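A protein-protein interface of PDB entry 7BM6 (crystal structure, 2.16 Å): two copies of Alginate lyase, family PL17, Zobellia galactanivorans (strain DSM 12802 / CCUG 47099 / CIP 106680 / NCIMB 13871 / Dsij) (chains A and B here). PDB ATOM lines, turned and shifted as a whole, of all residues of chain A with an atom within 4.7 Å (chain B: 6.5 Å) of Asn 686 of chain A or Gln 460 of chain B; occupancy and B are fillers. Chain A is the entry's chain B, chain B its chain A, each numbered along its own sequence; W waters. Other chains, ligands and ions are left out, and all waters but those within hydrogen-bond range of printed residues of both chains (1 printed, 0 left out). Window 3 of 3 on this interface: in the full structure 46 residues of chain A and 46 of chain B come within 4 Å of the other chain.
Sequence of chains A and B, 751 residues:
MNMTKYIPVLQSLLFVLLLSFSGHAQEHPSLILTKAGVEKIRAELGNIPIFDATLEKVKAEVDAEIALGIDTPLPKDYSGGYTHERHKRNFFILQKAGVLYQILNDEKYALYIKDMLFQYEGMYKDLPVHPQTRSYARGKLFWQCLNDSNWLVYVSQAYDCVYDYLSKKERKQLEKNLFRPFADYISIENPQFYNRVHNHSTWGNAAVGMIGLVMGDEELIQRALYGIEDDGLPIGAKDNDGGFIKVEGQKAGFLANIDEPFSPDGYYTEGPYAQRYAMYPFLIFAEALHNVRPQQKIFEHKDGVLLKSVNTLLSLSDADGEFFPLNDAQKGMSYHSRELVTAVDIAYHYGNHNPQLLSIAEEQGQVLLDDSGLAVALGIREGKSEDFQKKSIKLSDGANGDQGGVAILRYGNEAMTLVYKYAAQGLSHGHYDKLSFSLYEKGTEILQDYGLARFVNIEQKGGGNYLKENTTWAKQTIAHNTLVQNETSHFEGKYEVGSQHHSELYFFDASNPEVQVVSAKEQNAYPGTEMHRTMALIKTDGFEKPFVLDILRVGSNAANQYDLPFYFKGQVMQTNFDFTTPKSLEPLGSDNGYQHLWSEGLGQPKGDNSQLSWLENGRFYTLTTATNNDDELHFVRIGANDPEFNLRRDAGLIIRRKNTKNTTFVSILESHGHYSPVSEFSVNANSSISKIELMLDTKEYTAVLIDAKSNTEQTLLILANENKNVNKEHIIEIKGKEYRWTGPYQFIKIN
Ile 458 of chain B touches Met 573 of chain A (CG2 to SD, 3.9 Å).
Gln 460 of chain B touches Met 573 of chain A.
Lys 461 of chain B touches Met 573 of chain A.
OE1 of Gln 574 of chain A touches CG of Gln 460 of chain B, 3.4 Å away.
Ala 685 of chain A touches Gln 460 of chain B (CB to OE1, 3.7 Å).
Water W1 bridges the side-chain amino group of Lys 461 of chain B (2.8 Å) and the backbone carbonyl oxygen of Met 573 of chain A (3.1 Å).
NE2 of Gln 460 of chain B sits close to ND2 of Asn 686 of chain A, at 3.0 Å.
No position is printed for both chains.
Asn 686 of chain A touches just one residue of chain B: Gln 460 (3.0 Å).
Gln 460 of chain B touches four residues of chain A.
Printed residues of chain A within 4 Å of Lys 461 of chain B: Met 573 (3.9 Å).
Of the printed residues of chain B, Gln 574 of chain A touches Gln 460.
Of the printed residues of chain A, Ile 458 of chain B touches Met 573.
Of the printed residues of chain B, Ala 685 of chain A touches Gln 460 (3.7 Å).
The nearest printed residue of chain B that does not touch Gln 574 of chain A is Lys 461 of chain B (5.6 Å).
The backbone carbonyl oxygen (O) of Ile 458 of chain B lies within hydrogen-bond range of the backbone NH (N) of Gly 464 of chain B (3.2 Å).
The side-chain amide nitrogen (ND2) of Asn 686 of chain A sits at hydrogen-bond distance from the side-chain amide oxygen (OE1) of Gln 574 of chain A (2.9 Å).
A ring nitrogen (ND1) of His 672 of chain A sits at hydrogen-bond distance from the backbone carbonyl oxygen (O) of Asn 686 of chain A (3.2 Å).
Of the 9 printed residues of chain A, 4 touch a printed residue of chain B.
Hydrophobic or aromatic side chains of chain A within 4 Å of the printed part of chain B: Met 573 and Ala 685.
Hydrophobic or aromatic side chains of chain B that line the printed part of chain A: Ile 458.
Among the printed residues, 6 pairs touch across the chains.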
ATOM      1  N   MET A 573     -10.124 -19.829  -3.697  1.00  0.00           N
ATOM      2  CA  MET A 573     -10.758 -18.550  -4.029  1.00  0.00           C
ATOM      3  C   MET A 573     -10.163 -17.796  -5.248  1.00  0.00           C
ATOM      4  O   MET A 573     -10.902 -17.180  -6.002  1.00  0.00           O
ATOM      5  CB  MET A 573     -10.696 -17.605  -2.823  1.00  0.00           C
ATOM      6  CG  MET A 573     -11.611 -17.932  -1.646  1.00  0.00           C
ATOM      7  SD  MET A 573     -13.315 -17.565  -2.004  1.00  0.00           S
ATOM      8  CE  MET A 573     -14.004 -19.223  -1.972  1.00  0.00           C
ATOM      9  N   GLN A 574      -8.860 -17.699  -5.324  1.00  0.00           N
ATOM     10  CA  GLN A 574      -8.186 -16.994  -6.394  1.00  0.00           C
ATOM     11  C   GLN A 574      -6.703 -17.354  -6.516  1.00  0.00           C
ATOM     12  O   GLN A 574      -6.098 -17.819  -5.555  1.00  0.00           O
ATOM     13  CB  GLN A 574      -8.317 -15.456  -6.280  1.00  0.00           C
ATOM     14  CG  GLN A 574      -7.705 -14.855  -5.047  1.00  0.00           C
ATOM     15  CD  GLN A 574      -7.689 -13.314  -4.990  1.00  0.00           C
ATOM     16  OE1 GLN A 574      -7.835 -12.688  -3.881  1.00  0.00           O
ATOM     17  NE2 GLN A 574      -7.518 -12.686  -6.143  1.00  0.00           N
ATOM     18  N   HIS A 672      -6.293 -13.228   6.603  1.00  0.00           N
ATOM     19  CA  HIS A 672      -6.939 -11.930   6.542  1.00  0.00           C
ATOM     20  C   HIS A 672      -8.424 -12.068   6.305  1.00  0.00           C
ATOM     21  O   HIS A 672      -8.862 -12.958   5.568  1.00  0.00           O
ATOM     22  CB  HIS A 672      -6.338 -11.027   5.421  1.00  0.00           C
ATOM     23  CG  HIS A 672      -6.217 -11.734   4.104  1.00  0.00           C
ATOM     24  ND1 HIS A 672      -7.240 -11.760   3.178  1.00  0.00           N
ATOM     25  CD2 HIS A 672      -5.241 -12.524   3.600  1.00  0.00           C
ATOM     26  CE1 HIS A 672      -6.871 -12.498   2.140  1.00  0.00           C
ATOM     27  NE2 HIS A 672      -5.686 -12.997   2.381  1.00  0.00           N
ATOM     28  N   ASN A 684     -12.080  -7.839   3.802  1.00  0.00           N
ATOM     29  CA  ASN A 684     -10.565  -7.931   3.681  1.00  0.00           C
ATOM     30  C   ASN A 684     -10.144  -9.235   3.052  1.00  0.00           C
ATOM     31  O   ASN A 684      -9.327  -9.975   3.620  1.00  0.00           O
ATOM     32  CB  ASN A 684      -9.778  -7.661   5.011  1.00  0.00           C
ATOM     33  CG  ASN A 684      -8.230  -7.441   4.806  1.00  0.00           C
ATOM     34  OD1 ASN A 684      -7.776  -7.226   3.696  1.00  0.00           O
ATOM     35  ND2 ASN A 684      -7.430  -7.499   5.899  1.00  0.00           N
ATOM     36  N   ALA A 685     -10.688  -9.486   1.851  1.00  0.00           N
ATOM     37  CA  ALA A 685     -10.518 -10.760   1.140  1.00  0.00           C
ATOM     38  C   ALA A 685      -9.275 -10.815   0.282  1.00  0.00           C
ATOM     39  O   ALA A 685      -8.885 -11.883  -0.151  1.00  0.00           O
ATOM     40  CB  ALA A 685     -11.762 -11.108   0.294  1.00  0.00           C
ATOM     41  N   ASN A 686      -8.618  -9.693   0.069  1.00  0.00           N
ATOM     42  CA  ASN A 686      -7.364  -9.694  -0.724  1.00  0.00           C
ATOM     43  C   ASN A 686      -6.138  -9.726   0.165  1.00  0.00           C
ATOM     44  O   ASN A 686      -6.182  -9.329   1.339  1.00  0.00           O
ATOM     45  CB  ASN A 686      -7.317  -8.467  -1.660  1.00  0.00           C
ATOM     46  CG  ASN A 686      -8.204  -8.602  -2.918  1.00  0.00           C
ATOM     47  OD1 ASN A 686      -8.749  -7.606  -3.353  1.00  0.00           O
ATOM     48  ND2 ASN A 686      -8.288  -9.798  -3.551  1.00  0.00           N
ATOM     49  N   SER A 687      -5.032 -10.217  -0.390  1.00  0.00           N
ATOM     50  CA  SER A 687      -3.715 -10.120   0.235  1.00  0.00           C
ATOM     51  C   SER A 687      -3.318  -8.622   0.475  1.00  0.00           C
ATOM     52  O   SER A 687      -3.700  -7.746  -0.286  1.00  0.00           O
ATOM     53  CB  SER A 687      -2.686 -10.803  -0.649  1.00  0.00           C
ATOM     54  OG  SER A 687      -1.313 -10.624  -0.229  1.00  0.00           O
ATOM     55  N   SER A 688      -2.503  -8.386   1.485  1.00  0.00           N
ATOM     56  CA  SER A 688      -1.819  -7.113   1.669  1.00  0.00           C
ATOM     57  C   SER A 688      -0.317  -7.139   1.236  1.00  0.00           C
ATOM     58  O   SER A 688       0.399  -6.156   1.471  1.00  0.00           O
ATOM     59  CB  SER A 688      -1.898  -6.708   3.141  1.00  0.00           C
ATOM     60  OG  SER A 688      -3.226  -6.505   3.514  1.00  0.00           O
ATOM     61  N   LYS A 709       1.207  -3.969   0.658  1.00  0.00           N
ATOM     62  CA  LYS A 709       0.341  -3.183  -0.212  1.00  0.00           C
ATOM     63  C   LYS A 709      -0.313  -2.034   0.549  1.00  0.00           C
ATOM     64  O   LYS A 709      -1.152  -1.314   0.006  1.00  0.00           O
ATOM     65  CB  LYS A 709      -0.732  -4.072  -0.846  1.00  0.00           C
ATOM     66  CG  LYS A 709      -0.316  -4.704  -2.164  1.00  0.00           C
ATOM     67  CD  LYS A 709      -1.085  -5.987  -2.428  1.00  0.00           C
ATOM     68  CE  LYS A 709      -2.475  -5.695  -2.969  1.00  0.00           C
ATOM     69  NZ  LYS A 709      -3.383  -6.869  -2.834  1.00  0.00           N
ATOM     70  N   SER B  79     -20.598  -7.142  -6.430  1.00  0.00           N
ATOM     71  CA  SER B  79     -20.691  -7.450  -5.029  1.00  0.00           C
ATOM     72  C   SER B  79     -19.323  -7.892  -4.424  1.00  0.00           C
ATOM     73  O   SER B  79     -18.489  -8.547  -5.051  1.00  0.00           O
ATOM     74  CB  SER B  79     -21.766  -8.533  -4.777  1.00  0.00           C
ATOM     75  OG  SER B  79     -21.314  -9.819  -5.175  1.00  0.00           O
ATOM     76  N   GLY B  80     -19.077  -7.444  -3.196  1.00  0.00           N
ATOM     77  CA  GLY B  80     -17.790  -7.630  -2.603  1.00  0.00           C
ATOM     78  C   GLY B  80     -16.751  -6.603  -2.927  1.00  0.00           C
ATOM     79  O   GLY B  80     -15.797  -6.435  -2.138  1.00  0.00           O
ATOM     80  N   ASN B 457     -21.609 -12.752  -2.768  1.00  0.00           N
ATOM     81  CA  ASN B 457     -20.917 -11.503  -2.434  1.00  0.00           C
ATOM     82  C   ASN B 457     -19.410 -11.622  -2.217  1.00  0.00           C
ATOM     83  O   ASN B 457     -18.774 -10.690  -1.644  1.00  0.00           O
ATOM     84  CB  ASN B 457     -21.527 -10.749  -1.221  1.00  0.00           C
ATOM     85  CG  ASN B 457     -22.984 -10.444  -1.361  1.00  0.00           C
ATOM     86  OD1 ASN B 457     -23.516 -10.211  -2.474  1.00  0.00           O
ATOM     87  ND2 ASN B 457     -23.657 -10.399  -0.220  1.00  0.00           N
ATOM     88  N   ILE B 458     -18.812 -12.712  -2.696  1.00  0.00           N
ATOM     89  CA  ILE B 458     -17.351 -12.848  -2.672  1.00  0.00           C
ATOM     90  C   ILE B 458     -16.873 -12.482  -4.072  1.00  0.00           C
ATOM     91  O   ILE B 458     -17.006 -13.295  -5.028  1.00  0.00           O
ATOM     92  CB  ILE B 458     -16.861 -14.238  -2.264  1.00  0.00           C
ATOM     93  CG1 ILE B 458     -17.456 -14.608  -0.886  1.00  0.00           C
ATOM     94  CG2 ILE B 458     -15.342 -14.247  -2.235  1.00  0.00           C
ATOM     95  CD1 ILE B 458     -16.972 -15.879  -0.279  1.00  0.00           C
ATOM     96  N   GLU B 459     -16.293 -11.282  -4.173  1.00  0.00           N
ATOM     97  CA  GLU B 459     -15.866 -10.718  -5.463  1.00  0.00           C
ATOM     98  C   GLU B 459     -14.953 -11.583  -6.342  1.00  0.00           C
ATOM     99  O   GLU B 459     -15.065 -11.552  -7.550  1.00  0.00           O
ATOM    100  CB  GLU B 459     -15.128  -9.390  -5.233  1.00  0.00           C
ATOM    101  CG  GLU B 459     -15.003  -8.537  -6.509  1.00  0.00           C
ATOM    102  CD  GLU B 459     -14.231  -7.220  -6.293  1.00  0.00           C
ATOM    103  OE1 GLU B 459     -13.529  -7.123  -5.281  1.00  0.00           O
ATOM    104  OE2 GLU B 459     -14.408  -6.267  -7.084  1.00  0.00           O
ATOM    105  N   GLN B 460     -14.037 -12.299  -5.699  1.00  0.00           N
ATOM    106  CA  GLN B 460     -13.049 -13.116  -6.355  1.00  0.00           C
ATOM    107  C   GLN B 460     -13.697 -14.323  -7.044  1.00  0.00           C
ATOM    108  O   GLN B 460     -13.056 -14.949  -7.823  1.00  0.00           O
ATOM    109  CB  GLN B 460     -12.051 -13.600  -5.317  1.00  0.00           C
ATOM    110  CG  GLN B 460     -11.134 -12.488  -4.733  1.00  0.00           C
ATOM    111  CD  GLN B 460     -11.824 -11.524  -3.732  1.00  0.00           C
ATOM    112  OE1 GLN B 460     -12.902 -11.783  -3.139  1.00  0.00           O
ATOM    113  NE2 GLN B 460     -11.239 -10.391  -3.599  1.00  0.00           N
ATOM    114  N   LYS B 461     -14.936 -14.688  -6.670  1.00  0.00           N
ATOM    115  CA  LYS B 461     -15.658 -15.751  -7.309  1.00  0.00           C
ATOM    116  C   LYS B 461     -16.718 -15.156  -8.232  1.00  0.00           C
ATOM    117  O   LYS B 461     -17.906 -15.079  -7.871  1.00  0.00           O
ATOM    118  CB  LYS B 461     -16.306 -16.696  -6.248  1.00  0.00           C
ATOM    119  CG  LYS B 461     -15.312 -17.531  -5.465  1.00  0.00           C
ATOM    120  CD  LYS B 461     -14.527 -18.418  -6.437  1.00  0.00           C
ATOM    121  CE  LYS B 461     -14.572 -19.857  -6.127  1.00  0.00           C
ATOM    122  NZ  LYS B 461     -13.485 -20.532  -6.887  1.00  0.00           N
ATOM    123  N   GLY B 462     -16.271 -14.801  -9.445  1.00  0.00           N
ATOM    124  CA  GLY B 462     -17.107 -14.243 -10.499  1.00  0.00           C
ATOM    125  C   GLY B 462     -17.996 -13.082 -10.022  1.00  0.00           C
ATOM    126  O   GLY B 462     -19.188 -13.047 -10.239  1.00  0.00           O
ATOM    127  N   GLY B 463     -17.412 -12.178  -9.288  1.00  0.00           N
ATOM    128  CA  GLY B 463     -18.133 -10.971  -8.829  1.00  0.00           C
ATOM    129  C   GLY B 463     -19.213 -11.258  -7.765  1.00  0.00           C
ATOM    130  O   GLY B 463     -20.104 -10.408  -7.500  1.00  0.00           O
ATOM    131  N   GLY B 464     -19.171 -12.449  -7.189  1.00  0.00           N
ATOM    132  CA  GLY B 464     -20.116 -12.812  -6.116  1.00  0.00           C
ATOM    133  C   GLY B 464     -21.447 -13.268  -6.641  1.00  0.00           C
ATOM    134  O   GLY B 464     -22.388 -13.412  -5.861  1.00  0.00           O
HETATM  135  O   HOH W   1     -12.069 -18.734  -8.421  1.00  0.00           O
